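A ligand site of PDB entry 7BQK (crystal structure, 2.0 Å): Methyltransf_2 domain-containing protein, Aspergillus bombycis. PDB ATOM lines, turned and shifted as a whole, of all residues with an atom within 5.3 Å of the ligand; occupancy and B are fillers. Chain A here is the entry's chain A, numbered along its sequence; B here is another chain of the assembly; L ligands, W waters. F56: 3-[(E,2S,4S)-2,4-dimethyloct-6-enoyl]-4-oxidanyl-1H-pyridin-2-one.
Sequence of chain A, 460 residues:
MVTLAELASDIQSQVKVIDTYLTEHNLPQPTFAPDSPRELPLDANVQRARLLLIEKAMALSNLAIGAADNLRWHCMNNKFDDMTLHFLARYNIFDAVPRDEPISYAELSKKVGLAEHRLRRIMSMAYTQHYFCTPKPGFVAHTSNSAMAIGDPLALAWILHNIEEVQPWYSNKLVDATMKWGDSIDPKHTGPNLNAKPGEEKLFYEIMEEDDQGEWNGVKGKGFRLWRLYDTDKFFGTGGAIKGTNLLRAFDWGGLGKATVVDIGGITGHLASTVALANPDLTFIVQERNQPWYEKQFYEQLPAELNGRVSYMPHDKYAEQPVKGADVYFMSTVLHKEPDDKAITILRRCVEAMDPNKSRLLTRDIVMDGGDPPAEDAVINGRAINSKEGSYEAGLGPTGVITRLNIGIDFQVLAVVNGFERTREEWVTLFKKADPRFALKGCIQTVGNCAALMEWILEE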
ATOM      1  N   TRP A 158      -5.448   4.354   9.425  1.00  0.00           N
ATOM      2  CA  TRP A 158      -4.967   3.880  10.716  1.00  0.00           C
ATOM      3  C   TRP A 158      -4.149   2.608  10.577  1.00  0.00           C
ATOM      4  O   TRP A 158      -3.089   2.462  11.202  1.00  0.00           O
ATOM      5  CB  TRP A 158      -6.146   3.662  11.667  1.00  0.00           C
ATOM      6  CG  TRP A 158      -5.769   3.321  13.093  1.00  0.00           C
ATOM      7  CD1 TRP A 158      -6.246   2.272  13.837  1.00  0.00           C
ATOM      8  CD2 TRP A 158      -4.865   4.024  13.947  1.00  0.00           C
ATOM      9  NE1 TRP A 158      -5.684   2.276  15.092  1.00  0.00           N
ATOM     10  CE2 TRP A 158      -4.826   3.346  15.181  1.00  0.00           C
ATOM     11  CE3 TRP A 158      -4.063   5.161  13.785  1.00  0.00           C
ATOM     12  CZ2 TRP A 158      -4.043   3.762  16.249  1.00  0.00           C
ATOM     13  CZ3 TRP A 158      -3.284   5.595  14.839  1.00  0.00           C
ATOM     14  CH2 TRP A 158      -3.278   4.899  16.068  1.00  0.00           C
ATOM     15  N   HIS A 161      -0.736   3.717   8.654  1.00  0.00           N
ATOM     16  CA  HIS A 161       0.168   4.538   9.457  1.00  0.00           C
ATOM     17  C   HIS A 161       0.945   3.669  10.436  1.00  0.00           C
ATOM     18  O   HIS A 161       2.171   3.806  10.579  1.00  0.00           O
ATOM     19  CB  HIS A 161      -0.609   5.631  10.194  1.00  0.00           C
ATOM     20  CG  HIS A 161       0.169   6.344  11.257  1.00  0.00           C
ATOM     21  ND1 HIS A 161       1.359   6.994  10.993  1.00  0.00           N
ATOM     22  CD2 HIS A 161      -0.085   6.547  12.573  1.00  0.00           C
ATOM     23  CE1 HIS A 161       1.812   7.554  12.116  1.00  0.00           C
ATOM     24  NE2 HIS A 161       0.950   7.293  13.087  1.00  0.00           N
ATOM     25  N   VAL A 166       4.829   3.627  11.889  1.00  0.00           N
ATOM     26  CA  VAL A 166       5.157   3.575  13.314  1.00  0.00           C
ATOM     27  C   VAL A 166       5.980   2.333  13.637  1.00  0.00           C
ATOM     28  O   VAL A 166       7.032   2.396  14.267  1.00  0.00           O
ATOM     29  CB  VAL A 166       3.884   3.629  14.165  1.00  0.00           C
ATOM     30  CG1 VAL A 166       4.267   3.551  15.656  1.00  0.00           C
ATOM     31  CG2 VAL A 166       3.119   4.896  13.889  1.00  0.00           C
ATOM     32  N   PHE A 204      10.095  13.074  13.216  1.00  0.00           N
ATOM     33  CA  PHE A 204       8.886  12.432  12.689  1.00  0.00           C
ATOM     34  C   PHE A 204       8.012  13.413  11.918  1.00  0.00           C
ATOM     35  O   PHE A 204       7.617  13.142  10.782  1.00  0.00           O
ATOM     36  CB  PHE A 204       8.102  11.769  13.837  1.00  0.00           C
ATOM     37  CG  PHE A 204       6.702  11.364  13.469  1.00  0.00           C
ATOM     38  CD1 PHE A 204       6.471  10.216  12.725  1.00  0.00           C
ATOM     39  CD2 PHE A 204       5.609  12.105  13.899  1.00  0.00           C
ATOM     40  CE1 PHE A 204       5.186   9.834  12.391  1.00  0.00           C
ATOM     41  CE2 PHE A 204       4.310  11.723  13.583  1.00  0.00           C
ATOM     42  CZ  PHE A 204       4.108  10.579  12.827  1.00  0.00           C
ATOM     43  N   TYR A 205       7.695  14.562  12.515  1.00  0.00           N
ATOM     44  CA  TYR A 205       6.816  15.501  11.823  1.00  0.00           C
ATOM     45  C   TYR A 205       7.471  16.114  10.599  1.00  0.00           C
ATOM     46  O   TYR A 205       6.775  16.548   9.678  1.00  0.00           O
ATOM     47  CB  TYR A 205       6.314  16.581  12.795  1.00  0.00           C
ATOM     48  CG  TYR A 205       5.098  16.089  13.549  1.00  0.00           C
ATOM     49  CD1 TYR A 205       3.869  15.977  12.908  1.00  0.00           C
ATOM     50  CD2 TYR A 205       5.195  15.667  14.881  1.00  0.00           C
ATOM     51  CE1 TYR A 205       2.754  15.501  13.571  1.00  0.00           C
ATOM     52  CE2 TYR A 205       4.078  15.181  15.553  1.00  0.00           C
ATOM     53  CZ  TYR A 205       2.868  15.097  14.883  1.00  0.00           C
ATOM     54  OH  TYR A 205       1.736  14.614  15.515  1.00  0.00           O
ATOM     55  N   LEU A 229      -1.853  10.973   8.406  1.00  0.00           N
ATOM     56  CA  LEU A 229      -1.857  11.092   9.863  1.00  0.00           C
ATOM     57  C   LEU A 229      -3.067  11.892  10.335  1.00  0.00           C
ATOM     58  O   LEU A 229      -3.720  11.525  11.312  1.00  0.00           O
ATOM     59  CB  LEU A 229      -0.550  11.732  10.342  1.00  0.00           C
ATOM     60  CG  LEU A 229      -0.399  11.821  11.858  1.00  0.00           C
ATOM     61  CD1 LEU A 229      -0.267  10.420  12.465  1.00  0.00           C
ATOM     62  CD2 LEU A 229       0.813  12.650  12.231  1.00  0.00           C
ATOM     63  N   THR A 232      -6.015   9.667  10.457  1.00  0.00           N
ATOM     64  CA  THR A 232      -6.026   8.821  11.648  1.00  0.00           C
ATOM     65  C   THR A 232      -6.618   9.556  12.839  1.00  0.00           C
ATOM     66  O   THR A 232      -7.312   8.996  13.590  1.00  0.00           O
ATOM     67  CB  THR A 232      -4.659   8.225  11.978  1.00  0.00           C
ATOM     68  OG1 THR A 232      -3.782   9.189  12.511  1.00  0.00           O
ATOM     69  CG2 THR A 232      -4.048   7.485  10.774  1.00  0.00           C
ATOM     70  N   ASP A 233      -6.281  10.819  12.982  1.00  0.00           N
ATOM     71  CA  ASP A 233      -6.827  11.629  14.042  1.00  0.00           C
ATOM     72  C   ASP A 233      -8.353  11.684  13.917  1.00  0.00           C
ATOM     73  O   ASP A 233      -9.028  11.467  14.833  1.00  0.00           O
ATOM     74  CB  ASP A 233      -6.232  13.017  14.083  1.00  0.00           C
ATOM     75  CG  ASP A 233      -6.495  13.711  15.371  1.00  0.00           C
ATOM     76  OD1 ASP A 233      -7.510  14.306  15.478  1.00  0.00           O
ATOM     77  OD2 ASP A 233      -5.712  13.605  16.253  1.00  0.00           O
ATOM     78  N   PHE A 236     -10.224   8.463  15.049  1.00  0.00           N
ATOM     79  CA  PHE A 236     -10.512   8.340  16.447  1.00  0.00           C
ATOM     80  C   PHE A 236     -11.621   9.276  16.937  1.00  0.00           C
ATOM     81  O   PHE A 236     -12.173   9.064  17.984  1.00  0.00           O
ATOM     82  CB  PHE A 236      -9.260   8.378  17.284  1.00  0.00           C
ATOM     83  CG  PHE A 236      -8.529   7.073  17.303  1.00  0.00           C
ATOM     84  CD1 PHE A 236      -7.637   6.771  16.338  1.00  0.00           C
ATOM     85  CD2 PHE A 236      -8.780   6.127  18.271  1.00  0.00           C
ATOM     86  CE1 PHE A 236      -6.979   5.567  16.338  1.00  0.00           C
ATOM     87  CE2 PHE A 236      -8.121   4.929  18.278  1.00  0.00           C
ATOM     88  CZ  PHE A 236      -7.233   4.644  17.299  1.00  0.00           C
ATOM     89  N   ILE A 242     -12.807   7.246  21.975  1.00  0.00           N
ATOM     90  CA  ILE A 242     -12.401   8.657  22.039  1.00  0.00           C
ATOM     91  C   ILE A 242     -13.276   9.524  21.124  1.00  0.00           C
ATOM     92  O   ILE A 242     -12.857  10.633  20.749  1.00  0.00           O
ATOM     93  CB  ILE A 242     -10.915   8.828  21.699  1.00  0.00           C
ATOM     94  CG1 ILE A 242     -10.118   7.583  22.098  1.00  0.00           C
ATOM     95  CG2 ILE A 242     -10.352  10.046  22.429  1.00  0.00           C
ATOM     96  CD1 ILE A 242      -8.646   7.629  21.683  1.00  0.00           C
ATOM     97  N   THR A 333      -5.385  16.784  22.963  1.00  0.00           N
ATOM     98  CA  THR A 333      -4.280  15.830  22.788  1.00  0.00           C
ATOM     99  C   THR A 333      -3.080  16.477  22.104  1.00  0.00           C
ATOM    100  O   THR A 333      -2.438  15.890  21.217  1.00  0.00           O
ATOM    101  CB  THR A 333      -4.744  14.563  22.053  1.00  0.00           C
ATOM    102  OG1 THR A 333      -4.951  14.846  20.666  1.00  0.00           O
ATOM    103  CG2 THR A 333      -6.042  14.055  22.649  1.00  0.00           C
ATOM    104  N   HIS A 336       0.448  15.901  25.295  1.00  0.00           N
ATOM    105  CA  HIS A 336       1.147  14.640  25.513  1.00  0.00           C
ATOM    106  C   HIS A 336       2.303  14.427  24.545  1.00  0.00           C
ATOM    107  O   HIS A 336       3.050  13.452  24.714  1.00  0.00           O
ATOM    108  CB  HIS A 336       0.176  13.428  25.482  1.00  0.00           C
ATOM    109  CG  HIS A 336      -0.391  13.069  24.137  1.00  0.00           C
ATOM    110  ND1 HIS A 336      -0.701  11.768  23.790  1.00  0.00           N
ATOM    111  CD2 HIS A 336      -0.767  13.831  23.081  1.00  0.00           C
ATOM    112  CE1 HIS A 336      -1.223  11.738  22.577  1.00  0.00           C
ATOM    113  NE2 HIS A 336      -1.272  12.982  22.119  1.00  0.00           N
ATOM    114  N   LYS A 337       2.478  15.295  23.542  1.00  0.00           N
ATOM    115  CA  LYS A 337       3.664  15.307  22.706  1.00  0.00           C
ATOM    116  C   LYS A 337       4.598  16.439  23.075  1.00  0.00           C
ATOM    117  O   LYS A 337       5.560  16.712  22.343  1.00  0.00           O
ATOM    118  CB  LYS A 337       3.281  15.381  21.232  1.00  0.00           C
ATOM    119  CG  LYS A 337       2.769  14.014  20.705  1.00  0.00           C
ATOM    120  CD  LYS A 337       2.140  14.101  19.317  1.00  0.00           C
ATOM    121  CE  LYS A 337       0.829  14.854  19.364  1.00  0.00           C
ATOM    122  NZ  LYS A 337       0.263  14.926  18.002  1.00  0.00           N
ATOM    123  N   ASP A 365      -6.738  15.369  27.273  1.00  0.00           N
ATOM    124  CA  ASP A 365      -5.588  14.482  27.314  1.00  0.00           C
ATOM    125  C   ASP A 365      -5.852  13.302  28.248  1.00  0.00           C
ATOM    126  O   ASP A 365      -6.667  13.336  29.095  1.00  0.00           O
ATOM    127  CB  ASP A 365      -4.370  15.193  27.886  1.00  0.00           C
ATOM    128  CG  ASP A 365      -3.517  15.955  26.837  1.00  0.00           C
ATOM    129  OD1 ASP A 365      -3.066  15.407  25.864  1.00  0.00           O
ATOM    130  OD2 ASP A 365      -3.394  17.127  27.001  1.00  0.00           O
ATOM    131  N   ILE A 366      -5.064  12.281  28.070  1.00  0.00           N
ATOM    132  CA  ILE A 366      -5.071  11.172  28.936  1.00  0.00           C
ATOM    133  C   ILE A 366      -4.662  11.590  30.359  1.00  0.00           C
ATOM    134  O   ILE A 366      -3.740  12.316  30.550  1.00  0.00           O
ATOM    135  CB  ILE A 366      -4.075  10.113  28.419  1.00  0.00           C
ATOM    136  CG1 ILE A 366      -4.646   9.383  27.229  1.00  0.00           C
ATOM    137  CG2 ILE A 366      -3.756   9.108  29.486  1.00  0.00           C
ATOM    138  CD1 ILE A 366      -3.678   8.518  26.476  1.00  0.00           C
ATOM    139  N   ILE A 409      -1.237   4.396  23.633  1.00  0.00           N
ATOM    140  CA  ILE A 409      -1.076   5.777  23.181  1.00  0.00           C
ATOM    141  C   ILE A 409       0.237   6.362  23.707  1.00  0.00           C
ATOM    142  O   ILE A 409       0.984   7.000  22.956  1.00  0.00           O
ATOM    143  CB  ILE A 409      -2.287   6.614  23.620  1.00  0.00           C
ATOM    144  CG1 ILE A 409      -3.546   6.088  22.906  1.00  0.00           C
ATOM    145  CG2 ILE A 409      -2.075   8.110  23.312  1.00  0.00           C
ATOM    146  CD1 ILE A 409      -4.884   6.465  23.580  1.00  0.00           C
ATOM    147  N   GLN A 412       2.937   5.051  21.574  1.00  0.00           N
ATOM    148  CA  GLN A 412       2.919   5.643  20.250  1.00  0.00           C
ATOM    149  C   GLN A 412       3.616   7.006  20.250  1.00  0.00           C
ATOM    150  O   GLN A 412       4.458   7.280  19.395  1.00  0.00           O
ATOM    151  CB  GLN A 412       1.471   5.766  19.763  1.00  0.00           C
ATOM    152  CG  GLN A 412       1.357   6.100  18.281  1.00  0.00           C
ATOM    153  CD  GLN A 412       0.986   4.885  17.451  1.00  0.00           C
ATOM    154  OE1 GLN A 412       1.372   3.771  17.773  1.00  0.00           O
ATOM    155  NE2 GLN A 412       0.239   5.108  16.376  1.00  0.00           N
ATOM    156  N   VAL A 413       3.295   7.872  21.222  1.00  0.00           N
ATOM    157  CA  VAL A 413       3.957   9.170  21.220  1.00  0.00           C
ATOM    158  C   VAL A 413       5.393   9.020  21.707  1.00  0.00           C
ATOM    159  O   VAL A 413       6.261   9.792  21.299  1.00  0.00           O
ATOM    160  CB  VAL A 413       3.182  10.220  22.049  1.00  0.00           C
ATOM    161  CG1 VAL A 413       1.861  10.549  21.376  1.00  0.00           C
ATOM    162  CG2 VAL A 413       2.984   9.782  23.489  1.00  0.00           C
ATOM    163  N   VAL A 416       7.278   7.942  18.384  1.00  0.00           N
ATOM    164  CA  VAL A 416       7.510   8.894  17.293  1.00  0.00           C
ATOM    165  C   VAL A 416       8.178  10.191  17.752  1.00  0.00           C
ATOM    166  O   VAL A 416       8.929  10.784  16.972  1.00  0.00           O
ATOM    167  CB  VAL A 416       6.221   9.190  16.507  1.00  0.00           C
ATOM    168  CG1 VAL A 416       5.696   7.936  15.827  1.00  0.00           C
ATOM    169  CG2 VAL A 416       5.131   9.817  17.390  1.00  0.00           C
ATOM    170  N   GLU A 421       2.621  10.197  28.512  1.00  0.00           N
ATOM    171  CA  GLU A 421       1.361  10.533  29.177  1.00  0.00           C
ATOM    172  C   GLU A 421       1.628  10.849  30.642  1.00  0.00           C
ATOM    173  O   GLU A 421       2.650  10.458  31.206  1.00  0.00           O
ATOM    174  CB  GLU A 421       0.343   9.392  29.066  1.00  0.00           C
ATOM    175  CG  GLU A 421       0.082   8.882  27.664  1.00  0.00           C
ATOM    176  CD  GLU A 421      -0.390   9.965  26.697  1.00  0.00           C
ATOM    177  OE1 GLU A 421      -1.081  10.908  27.141  1.00  0.00           O
ATOM    178  OE2 GLU A 421      -0.074   9.865  25.493  1.00  0.00           O
ATOM    179  N   CYS A 450     -10.980   7.080  27.101  1.00  0.00           N
ATOM    180  CA  CYS A 450      -9.638   7.018  27.667  1.00  0.00           C
ATOM    181  C   CYS A 450      -9.042   8.390  27.953  1.00  0.00           C
ATOM    182  O   CYS A 450      -7.998   8.472  28.622  1.00  0.00           O
ATOM    183  CB  CYS A 450      -8.705   6.236  26.727  1.00  0.00           C
ATOM    184  SG  CYS A 450      -8.246   7.086  25.200  1.00  0.00           S
ATOM    185  N   ALA A 451      -9.661   9.460  27.480  1.00  0.00           N
ATOM    186  CA  ALA A 451      -9.191  10.830  27.688  1.00  0.00           C
ATOM    187  C   ALA A 451     -10.140  11.568  28.631  1.00  0.00           C
ATOM    188  O   ALA A 451     -11.316  11.225  28.768  1.00  0.00           O
ATOM    189  CB  ALA A 451      -9.097  11.582  26.359  1.00  0.00           C
ATOM    190  N   MET B  76      -3.534   0.097  17.538  1.00  0.00           N
ATOM    191  CA  MET B  76      -2.840   0.872  18.537  1.00  0.00           C
ATOM    192  C   MET B  76      -1.983  -0.031  19.379  1.00  0.00           C
ATOM    193  O   MET B  76      -0.838   0.145  19.465  1.00  0.00           O
ATOM    194  CB  MET B  76      -3.795   1.550  19.467  1.00  0.00           C
ATOM    195  CG  MET B  76      -3.131   2.465  20.444  1.00  0.00           C
ATOM    196  SD  MET B  76      -2.719   4.064  19.769  1.00  0.00           S
ATOM    197  CE  MET B  76      -4.316   4.785  19.691  1.00  0.00           C
HETATM  198  C1  F56 L   1       1.347  10.889  16.395  1.00  0.00           C
HETATM  199  C2  F56 L   1       1.519   9.880  15.462  1.00  0.00           C
HETATM  200  C4  F56 L   1      -0.341   8.718  16.334  1.00  0.00           C
HETATM  201  C5  F56 L   1      -0.540   9.729  17.285  1.00  0.00           C
HETATM  202  C6  F56 L   1       0.325  10.785  17.276  1.00  0.00           C
HETATM  203  C7  F56 L   1      -1.629   9.748  18.370  1.00  0.00           C
HETATM  204  C8  F56 L   1      -2.573   8.566  18.659  1.00  0.00           C
HETATM  205  C9  F56 L   1      -3.712   8.933  19.609  1.00  0.00           C
HETATM  206  C10 F56 L   1      -4.729   9.863  18.956  1.00  0.00           C
HETATM  207  C11 F56 L   1      -5.840  10.179  19.972  1.00  0.00           C
HETATM  208  C12 F56 L   1      -5.264  10.733  21.277  1.00  0.00           C
HETATM  209  C13 F56 L   1      -5.667  10.244  22.428  1.00  0.00           C
HETATM  210  C14 F56 L   1      -5.094  10.781  23.735  1.00  0.00           C
HETATM  211  C18 F56 L   1      -1.716   7.542  19.391  1.00  0.00           C
HETATM  212  C19 F56 L   1      -5.337   9.206  17.723  1.00  0.00           C
HETATM  213  N3  F56 L   1       0.689   8.822  15.465  1.00  0.00           N
HETATM  214  O15 F56 L   1       0.138  11.787  18.219  1.00  0.00           O
HETATM  215  O16 F56 L   1      -1.685  10.700  19.083  1.00  0.00           O
HETATM  216  O17 F56 L   1      -1.046   7.757  16.263  1.00  0.00           O
HETATM  217  O   HOH W   1      -2.998  12.169  16.605  1.00  0.00           O
HETATM  218  O   HOH W   2      -2.574  13.481  19.633  1.00  0.00           O
HETATM  219  O   HOH W   3      -3.131   9.673  15.178  1.00  0.00           O
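Water W2 lies within hydrogen-bond range of NE2 of His 336, O of Thr 333 and O16 of the ligand.
Water W3 bridges OG1 of Thr 232 (2.8 Å) and O17 of the ligand (3.0 Å).
Water W1 lies within hydrogen-bond range of OD2 of Asp 233 (3.1 Å) and O16 of the ligand (3.2 Å).
N3 of the ligand lies within hydrogen-bond range of NE2 of His 161 (2.8 Å).
NZ of Lys 337 is in hydrogen-bond range of O15 of the ligand, 3.1 Å away.
The side-chain amide nitrogen (NE2) of Gln 412 lies within hydrogen-bond range of an oxygen (O17) of the ligand (2.9 Å).
N of Val 166 lies within hydrogen-bond range of O of His 161.
A ring nitrogen (ND1) of His 336 is in hydrogen-bond range of the side-chain carboxylate (OE2) of Glu 421 (2.6 Å).
The side-chain hydroxyl of Thr 232 lies within hydrogen-bond range of the backbone carbonyl oxygen of Leu 229 (2.6 Å).
The backbone carbonyl oxygen (O) of Thr 333 sits close to a ring nitrogen (NE2) of His 336 (3.3 Å).
NZ of Lys 337 is in hydrogen-bond range of OH of Tyr 205 (2.9 Å).
Residues that only touch the ligand: Trp 158 (3.4 Å), Leu 229 (3.5 Å), Thr 333 (3.6 Å), Phe 236 (3.6 Å), Met 76 of chain B (3.6 Å), His 336 (3.7 Å), Phe 204 (3.8 Å), Ile 366 (3.8 Å), Val 413 (3.8 Å), Tyr 205 (3.8 Å) and Ile 409 (3.98 Å).
Hydrophobic or aromatic side chains that line the ligand: Trp 158, His 161, Phe 204, Leu 229, Phe 236, His 336, Ile 366, Ile 409, Val 413 and Met 76 of chain B.
Within 4 Å of the ligand: Trp 158, His 161, Phe 204, Tyr 205, Leu 229, Phe 236, Thr 333, His 336, Lys 337, Ile 366, Ile 409, Gln 412, Val 413 and Met 76 of chain B.
The nearest printed residue that does not touch the ligand is Ile 242 (4.03 Å).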
